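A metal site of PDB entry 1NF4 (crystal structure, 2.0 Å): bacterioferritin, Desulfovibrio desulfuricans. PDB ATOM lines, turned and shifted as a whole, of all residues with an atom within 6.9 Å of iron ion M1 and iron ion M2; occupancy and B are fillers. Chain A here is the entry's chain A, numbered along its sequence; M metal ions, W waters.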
ATOM      1  N   ALA A  19       1.124  26.110  17.366  1.00  0.00           N
ATOM      2  CA  ALA A  19       1.725  26.332  18.681  1.00  0.00           C
ATOM      3  C   ALA A  19       3.221  26.606  18.516  1.00  0.00           C
ATOM      4  O   ALA A  19       3.791  27.532  19.094  1.00  0.00           O
ATOM      5  CB  ALA A  19       1.501  25.135  19.584  1.00  0.00           C
ATOM      6  N   MET A  22       4.018  29.961  17.335  1.00  0.00           N
ATOM      7  CA  MET A  22       3.855  30.826  18.501  1.00  0.00           C
ATOM      8  C   MET A  22       5.105  30.778  19.381  1.00  0.00           C
ATOM      9  O   MET A  22       5.518  31.840  19.857  1.00  0.00           O
ATOM     10  CB  MET A  22       2.614  30.428  19.291  1.00  0.00           C
ATOM     11  CG  MET A  22       1.334  30.913  18.593  1.00  0.00           C
ATOM     12  SD  MET A  22      -0.126  30.237  19.391  1.00  0.00           S
ATOM     13  CE  MET A  22      -0.284  31.265  20.831  1.00  0.00           C
ATOM     14  N   GLU A  23       5.697  29.613  19.571  1.00  0.00           N
ATOM     15  CA  GLU A  23       6.944  29.502  20.337  1.00  0.00           C
ATOM     16  C   GLU A  23       8.078  30.250  19.642  1.00  0.00           C
ATOM     17  O   GLU A  23       8.846  30.985  20.260  1.00  0.00           O
ATOM     18  CB  GLU A  23       7.363  28.041  20.529  1.00  0.00           C
ATOM     19  CG  GLU A  23       6.409  27.186  21.348  1.00  0.00           C
ATOM     20  CD  GLU A  23       6.297  27.643  22.786  1.00  0.00           C
ATOM     21  OE1 GLU A  23       7.208  28.351  23.277  1.00  0.00           O
ATOM     22  OE2 GLU A  23       5.294  27.294  23.442  1.00  0.00           O
ATOM     23  N   ALA A  26       7.818  33.834  20.303  1.00  0.00           N
ATOM     24  CA  ALA A  26       8.181  34.162  21.678  1.00  0.00           C
ATOM     25  C   ALA A  26       9.686  34.158  21.899  1.00  0.00           C
ATOM     26  O   ALA A  26      10.228  35.007  22.595  1.00  0.00           O
ATOM     27  CB  ALA A  26       7.519  33.191  22.653  1.00  0.00           C
ATOM     28  N   TYR A  30      11.164  37.644  23.169  1.00  0.00           N
ATOM     29  CA  TYR A  30      11.808  37.630  24.477  1.00  0.00           C
ATOM     30  C   TYR A  30      13.302  37.891  24.355  1.00  0.00           C
ATOM     31  O   TYR A  30      13.879  38.609  25.176  1.00  0.00           O
ATOM     32  CB  TYR A  30      11.565  36.298  25.207  1.00  0.00           C
ATOM     33  CG  TYR A  30      10.094  36.067  25.525  1.00  0.00           C
ATOM     34  CD1 TYR A  30       9.634  34.802  25.855  1.00  0.00           C
ATOM     35  CD2 TYR A  30       9.195  37.125  25.479  1.00  0.00           C
ATOM     36  CE1 TYR A  30       8.292  34.584  26.138  1.00  0.00           C
ATOM     37  CE2 TYR A  30       7.852  36.930  25.768  1.00  0.00           C
ATOM     38  CZ  TYR A  30       7.418  35.659  26.094  1.00  0.00           C
ATOM     39  OH  TYR A  30       6.091  35.439  26.374  1.00  0.00           O
ATOM     40  N   ILE A  52      13.630  32.332  30.213  1.00  0.00           N
ATOM     41  CA  ILE A  52      12.288  32.008  29.709  1.00  0.00           C
ATOM     42  C   ILE A  52      12.329  31.779  28.203  1.00  0.00           C
ATOM     43  O   ILE A  52      11.672  30.856  27.713  1.00  0.00           O
ATOM     44  CB  ILE A  52      11.255  33.091  30.084  1.00  0.00           C
ATOM     45  CG1 ILE A  52      10.957  33.112  31.585  1.00  0.00           C
ATOM     46  CG2 ILE A  52       9.979  32.953  29.286  1.00  0.00           C
ATOM     47  CD1 ILE A  52      10.142  34.304  32.028  1.00  0.00           C
ATOM     48  N   ASP A  55      13.192  28.301  27.794  1.00  0.00           N
ATOM     49  CA  ASP A  55      12.032  27.433  27.977  1.00  0.00           C
ATOM     50  C   ASP A  55      11.200  27.382  26.682  1.00  0.00           C
ATOM     51  O   ASP A  55      10.699  26.335  26.323  1.00  0.00           O
ATOM     52  CB  ASP A  55      11.094  27.902  29.085  1.00  0.00           C
ATOM     53  CG  ASP A  55      11.596  27.734  30.492  1.00  0.00           C
ATOM     54  OD1 ASP A  55      12.610  27.054  30.742  1.00  0.00           O
ATOM     55  OD2 ASP A  55      10.934  28.301  31.412  1.00  0.00           O
ATOM     56  N   GLU A  56      11.043  28.520  25.993  1.00  0.00           N
ATOM     57  CA  GLU A  56      10.256  28.535  24.753  1.00  0.00           C
ATOM     58  C   GLU A  56      10.952  27.761  23.639  1.00  0.00           C
ATOM     59  O   GLU A  56      10.280  27.101  22.839  1.00  0.00           O
ATOM     60  CB  GLU A  56       9.966  29.960  24.275  1.00  0.00           C
ATOM     61  CG  GLU A  56       9.462  30.920  25.327  1.00  0.00           C
ATOM     62  CD  GLU A  56       8.146  30.579  25.981  1.00  0.00           C
ATOM     63  OE1 GLU A  56       7.702  29.419  26.047  1.00  0.00           O
ATOM     64  OE2 GLU A  56       7.499  31.511  26.499  1.00  0.00           O
ATOM     65  N   MET A  57      12.275  27.789  23.591  1.00  0.00           N
ATOM     66  CA  MET A  57      13.040  26.955  22.668  1.00  0.00           C
ATOM     67  C   MET A  57      12.748  25.478  22.923  1.00  0.00           C
ATOM     68  O   MET A  57      12.510  24.732  21.971  1.00  0.00           O
ATOM     69  CB  MET A  57      14.535  27.184  22.786  1.00  0.00           C
ATOM     70  CG  MET A  57      14.995  28.593  22.488  1.00  0.00           C
ATOM     71  SD  MET A  57      16.701  28.893  22.958  1.00  0.00           S
ATOM     72  CE  MET A  57      16.723  30.677  23.173  1.00  0.00           C
ATOM     73  N   HIS A  59      10.054  24.238  24.276  1.00  0.00           N
ATOM     74  CA  HIS A  59       8.677  23.965  23.854  1.00  0.00           C
ATOM     75  C   HIS A  59       8.634  23.752  22.351  1.00  0.00           C
ATOM     76  O   HIS A  59       8.002  22.844  21.813  1.00  0.00           O
ATOM     77  CB  HIS A  59       7.732  25.094  24.258  1.00  0.00           C
ATOM     78  CG  HIS A  59       7.563  25.297  25.730  1.00  0.00           C
ATOM     79  ND1 HIS A  59       6.959  26.415  26.267  1.00  0.00           N
ATOM     80  CD2 HIS A  59       7.939  24.526  26.791  1.00  0.00           C
ATOM     81  CE1 HIS A  59       6.965  26.313  27.594  1.00  0.00           C
ATOM     82  NE2 HIS A  59       7.550  25.180  27.925  1.00  0.00           N
ATOM     83  N   ALA A  60       9.344  24.602  21.619  1.00  0.00           N
ATOM     84  CA  ALA A  60       9.355  24.474  20.157  1.00  0.00           C
ATOM     85  C   ALA A  60       9.898  23.112  19.747  1.00  0.00           C
ATOM     86  O   ALA A  60       9.373  22.453  18.857  1.00  0.00           O
ATOM     87  CB  ALA A  60      10.182  25.583  19.532  1.00  0.00           C
ATOM     88  N   PHE A  63       7.253  20.350  20.610  1.00  0.00           N
ATOM     89  CA  PHE A  63       6.237  20.323  19.552  1.00  0.00           C
ATOM     90  C   PHE A  63       6.761  19.685  18.277  1.00  0.00           C
ATOM     91  O   PHE A  63       6.110  18.848  17.662  1.00  0.00           O
ATOM     92  CB  PHE A  63       5.743  21.745  19.267  1.00  0.00           C
ATOM     93  CG  PHE A  63       4.889  22.329  20.375  1.00  0.00           C
ATOM     94  CD1 PHE A  63       5.077  23.625  20.820  1.00  0.00           C
ATOM     95  CD2 PHE A  63       3.907  21.549  20.963  1.00  0.00           C
ATOM     96  CE1 PHE A  63       4.275  24.110  21.839  1.00  0.00           C
ATOM     97  CE2 PHE A  63       3.095  22.040  21.963  1.00  0.00           C
ATOM     98  CZ  PHE A  63       3.284  23.336  22.408  1.00  0.00           C
ATOM     99  N   GLN A  98       0.850  38.338  26.227  1.00  0.00           N
ATOM    100  CA  GLN A  98       1.146  37.240  25.294  1.00  0.00           C
ATOM    101  C   GLN A  98       1.063  35.882  25.966  1.00  0.00           C
ATOM    102  O   GLN A  98       0.442  34.969  25.406  1.00  0.00           O
ATOM    103  CB  GLN A  98       2.540  37.454  24.705  1.00  0.00           C
ATOM    104  CG  GLN A  98       2.936  36.432  23.650  1.00  0.00           C
ATOM    105  CD  GLN A  98       4.366  36.695  23.171  1.00  0.00           C
ATOM    106  OE1 GLN A  98       4.593  37.595  22.369  1.00  0.00           O
ATOM    107  NE2 GLN A  98       5.317  35.892  23.655  1.00  0.00           N
ATOM    108  N   GLU A  99       1.646  35.706  27.153  1.00  0.00           N
ATOM    109  CA  GLU A  99       1.565  34.446  27.884  1.00  0.00           C
ATOM    110  C   GLU A  99       0.105  34.040  28.091  1.00  0.00           C
ATOM    111  O   GLU A  99      -0.280  32.881  27.972  1.00  0.00           O
ATOM    112  CB  GLU A  99       2.272  34.523  29.239  1.00  0.00           C
ATOM    113  CG  GLU A  99       3.789  34.620  29.166  1.00  0.00           C
ATOM    114  CD  GLU A  99       4.443  33.367  28.618  1.00  0.00           C
ATOM    115  OE1 GLU A  99       3.798  32.301  28.628  1.00  0.00           O
ATOM    116  OE2 GLU A  99       5.610  33.419  28.155  1.00  0.00           O
ATOM    117  N   THR A 102      -1.301  32.950  24.910  1.00  0.00           N
ATOM    118  CA  THR A 102      -0.801  31.609  24.619  1.00  0.00           C
ATOM    119  C   THR A 102      -1.549  30.530  25.378  1.00  0.00           C
ATOM    120  O   THR A 102      -1.927  29.491  24.821  1.00  0.00           O
ATOM    121  CB  THR A 102       0.705  31.522  24.953  1.00  0.00           C
ATOM    122  OG1 THR A 102       1.389  32.365  24.022  1.00  0.00           O
ATOM    123  CG2 THR A 102       1.251  30.118  24.764  1.00  0.00           C
ATOM    124  N   TYR A 106      -3.387  27.459  23.493  1.00  0.00           N
ATOM    125  CA  TYR A 106      -2.947  26.096  23.729  1.00  0.00           C
ATOM    126  C   TYR A 106      -4.080  25.276  24.341  1.00  0.00           C
ATOM    127  O   TYR A 106      -4.210  24.092  24.064  1.00  0.00           O
ATOM    128  CB  TYR A 106      -1.726  26.055  24.655  1.00  0.00           C
ATOM    129  CG  TYR A 106      -0.440  26.520  24.011  1.00  0.00           C
ATOM    130  CD1 TYR A 106      -0.441  27.155  22.775  1.00  0.00           C
ATOM    131  CD2 TYR A 106       0.786  26.310  24.640  1.00  0.00           C
ATOM    132  CE1 TYR A 106       0.734  27.583  22.177  1.00  0.00           C
ATOM    133  CE2 TYR A 106       1.967  26.730  24.042  1.00  0.00           C
ATOM    134  CZ  TYR A 106       1.954  27.369  22.818  1.00  0.00           C
ATOM    135  OH  TYR A 106       3.129  27.785  22.233  1.00  0.00           O
ATOM    136  N   ILE A 128       2.997  21.796  28.862  1.00  0.00           N
ATOM    137  CA  ILE A 128       3.579  23.092  28.463  1.00  0.00           C
ATOM    138  C   ILE A 128       2.721  24.244  28.971  1.00  0.00           C
ATOM    139  O   ILE A 128       3.237  25.301  29.357  1.00  0.00           O
ATOM    140  CB  ILE A 128       3.810  23.085  26.932  1.00  0.00           C
ATOM    141  CG1 ILE A 128       4.958  22.163  26.513  1.00  0.00           C
ATOM    142  CG2 ILE A 128       4.033  24.490  26.391  1.00  0.00           C
ATOM    143  CD1 ILE A 128       5.174  21.980  25.040  1.00  0.00           C
ATOM    144  N   GLU A 131       3.775  25.342  32.319  1.00  0.00           N
ATOM    145  CA  GLU A 131       4.994  26.143  32.279  1.00  0.00           C
ATOM    146  C   GLU A 131       4.695  27.572  31.822  1.00  0.00           C
ATOM    147  O   GLU A 131       5.282  28.522  32.343  1.00  0.00           O
ATOM    148  CB  GLU A 131       6.033  25.491  31.361  1.00  0.00           C
ATOM    149  CG  GLU A 131       6.290  24.044  31.756  1.00  0.00           C
ATOM    150  CD  GLU A 131       7.479  23.423  31.052  1.00  0.00           C
ATOM    151  OE1 GLU A 131       7.931  23.941  30.013  1.00  0.00           O
ATOM    152  OE2 GLU A 131       7.961  22.379  31.534  1.00  0.00           O
ATOM    153  N   GLU A 132       3.781  27.710  30.857  1.00  0.00           N
ATOM    154  CA  GLU A 132       3.369  29.054  30.454  1.00  0.00           C
ATOM    155  C   GLU A 132       2.742  29.790  31.642  1.00  0.00           C
ATOM    156  O   GLU A 132       2.913  30.999  31.774  1.00  0.00           O
ATOM    157  CB  GLU A 132       2.397  29.043  29.283  1.00  0.00           C
ATOM    158  CG  GLU A 132       2.781  28.264  28.054  1.00  0.00           C
ATOM    159  CD  GLU A 132       4.057  28.675  27.378  1.00  0.00           C
ATOM    160  OE1 GLU A 132       4.747  29.584  27.864  1.00  0.00           O
ATOM    161  OE2 GLU A 132       4.416  28.086  26.333  1.00  0.00           O
ATOM    162  N   GLN A 133       2.040  29.055  32.500  1.00  0.00           N
ATOM    163  CA  GLN A 133       1.449  29.695  33.674  1.00  0.00           C
ATOM    164  C   GLN A 133       2.555  30.213  34.587  1.00  0.00           C
ATOM    165  O   GLN A 133       2.389  31.275  35.192  1.00  0.00           O
ATOM    166  CB  GLN A 133       0.532  28.744  34.438  1.00  0.00           C
ATOM    167  CG  GLN A 133       0.004  29.259  35.761  1.00  0.00           C
ATOM    168  CD  GLN A 133      -0.882  30.482  35.628  1.00  0.00           C
ATOM    169  OE1 GLN A 133      -1.977  30.432  35.071  1.00  0.00           O
ATOM    170  NE2 GLN A 133      -0.432  31.628  36.126  1.00  0.00           N
ATOM    171  N   HIS A 135       5.438  31.294  33.538  1.00  0.00           N
ATOM    172  CA  HIS A 135       5.893  32.492  32.848  1.00  0.00           C
ATOM    173  C   HIS A 135       4.956  33.672  33.090  1.00  0.00           C
ATOM    174  O   HIS A 135       5.408  34.758  33.452  1.00  0.00           O
ATOM    175  CB  HIS A 135       6.032  32.243  31.336  1.00  0.00           C
ATOM    176  CG  HIS A 135       7.027  31.184  30.975  1.00  0.00           C
ATOM    177  ND1 HIS A 135       7.094  30.615  29.725  1.00  0.00           N
ATOM    178  CD2 HIS A 135       7.996  30.588  31.705  1.00  0.00           C
ATOM    179  CE1 HIS A 135       8.049  29.713  29.679  1.00  0.00           C
ATOM    180  NE2 HIS A 135       8.614  29.681  30.880  1.00  0.00           N
ATOM    181  N   LEU A 136       3.650  33.473  32.880  1.00  0.00           N
ATOM    182  CA  LEU A 136       2.650  34.515  33.101  1.00  0.00           C
ATOM    183  C   LEU A 136       2.789  35.127  34.480  1.00  0.00           C
ATOM    184  O   LEU A 136       2.908  36.338  34.653  1.00  0.00           O
ATOM    185  CB  LEU A 136       1.255  33.920  32.910  1.00  0.00           C
ATOM    186  CG  LEU A 136       0.025  34.762  33.243  1.00  0.00           C
ATOM    187  CD1 LEU A 136       0.088  36.131  32.573  1.00  0.00           C
ATOM    188  CD2 LEU A 136      -1.239  34.036  32.810  1.00  0.00           C
ATOM    189  N   TYR A 139       5.831  37.361  34.713  1.00  0.00           N
ATOM    190  CA  TYR A 139       5.735  38.684  34.069  1.00  0.00           C
ATOM    191  C   TYR A 139       4.776  39.591  34.824  1.00  0.00           C
ATOM    192  O   TYR A 139       4.989  40.804  34.937  1.00  0.00           O
ATOM    193  CB  TYR A 139       5.314  38.520  32.610  1.00  0.00           C
ATOM    194  CG  TYR A 139       6.390  37.966  31.702  1.00  0.00           C
ATOM    195  CD1 TYR A 139       6.134  36.885  30.861  1.00  0.00           C
ATOM    196  CD2 TYR A 139       7.662  38.512  31.687  1.00  0.00           C
ATOM    197  CE1 TYR A 139       7.116  36.377  30.037  1.00  0.00           C
ATOM    198  CE2 TYR A 139       8.660  38.015  30.858  1.00  0.00           C
ATOM    199  CZ  TYR A 139       8.380  36.943  30.040  1.00  0.00           C
ATOM    200  OH  TYR A 139       9.360  36.434  29.206  1.00  0.00           O
HETATM  201 FE    FE M   1       5.905  31.270  27.899  1.00  0.00          FE
HETATM  202 FE    FE M   2       6.157  28.249  25.275  1.00  0.00          FE
HETATM  203  O   HOH W   1       5.477  30.285  24.233  1.00  0.00           O
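NE2 of His 59 sits at hydrogen-bond distance from OE1 of Glu 131, 2.5 Å away.
The side-chain carboxylate (OE2) of Glu 23 lies close to the side-chain hydroxyl (OH) of Tyr 106, at 2.5 Å.
NE2 of His 135 lies within hydrogen-bond range of OD2 of Asp 55, at 2.8 Å.
The side-chain carboxylate (OE2) of Glu 99 lies close to the side-chain hydroxyl (OH) of Tyr 30.
Within 4 Å of iron ion M1: Glu 56, Glu 99, Glu 132 and His 135.
Along chain A the residues within 4 Å of iron ion M2 span positions 23 to 132.
OE1 of Glu 132 binds iron ion M1 (2.0 Å).
The side-chain carboxylate (OE2) of Glu 56 binds iron ion M1 (2.1 Å).
Iron ion M1 is bound by OE2 of Glu 99 (2.2 Å).
Iron ion M1 is bound by a ring nitrogen (ND1) of His 135.
The side-chain carboxylate (OE1) of Glu 99 binds iron ion M1, 2.5 Å away.
Iron ion M1 has five donor atoms within binding distance.
Iron ion M2 is bound by the side-chain carboxylate (OE2) of Glu 132, the side-chain carboxylate (OE1) of Glu 56, a ring nitrogen (ND1) of His 59, the side-chain carboxylate (OE2) of Glu 23, the side-chain carboxylate (OE1) of Glu 23 and water W1.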
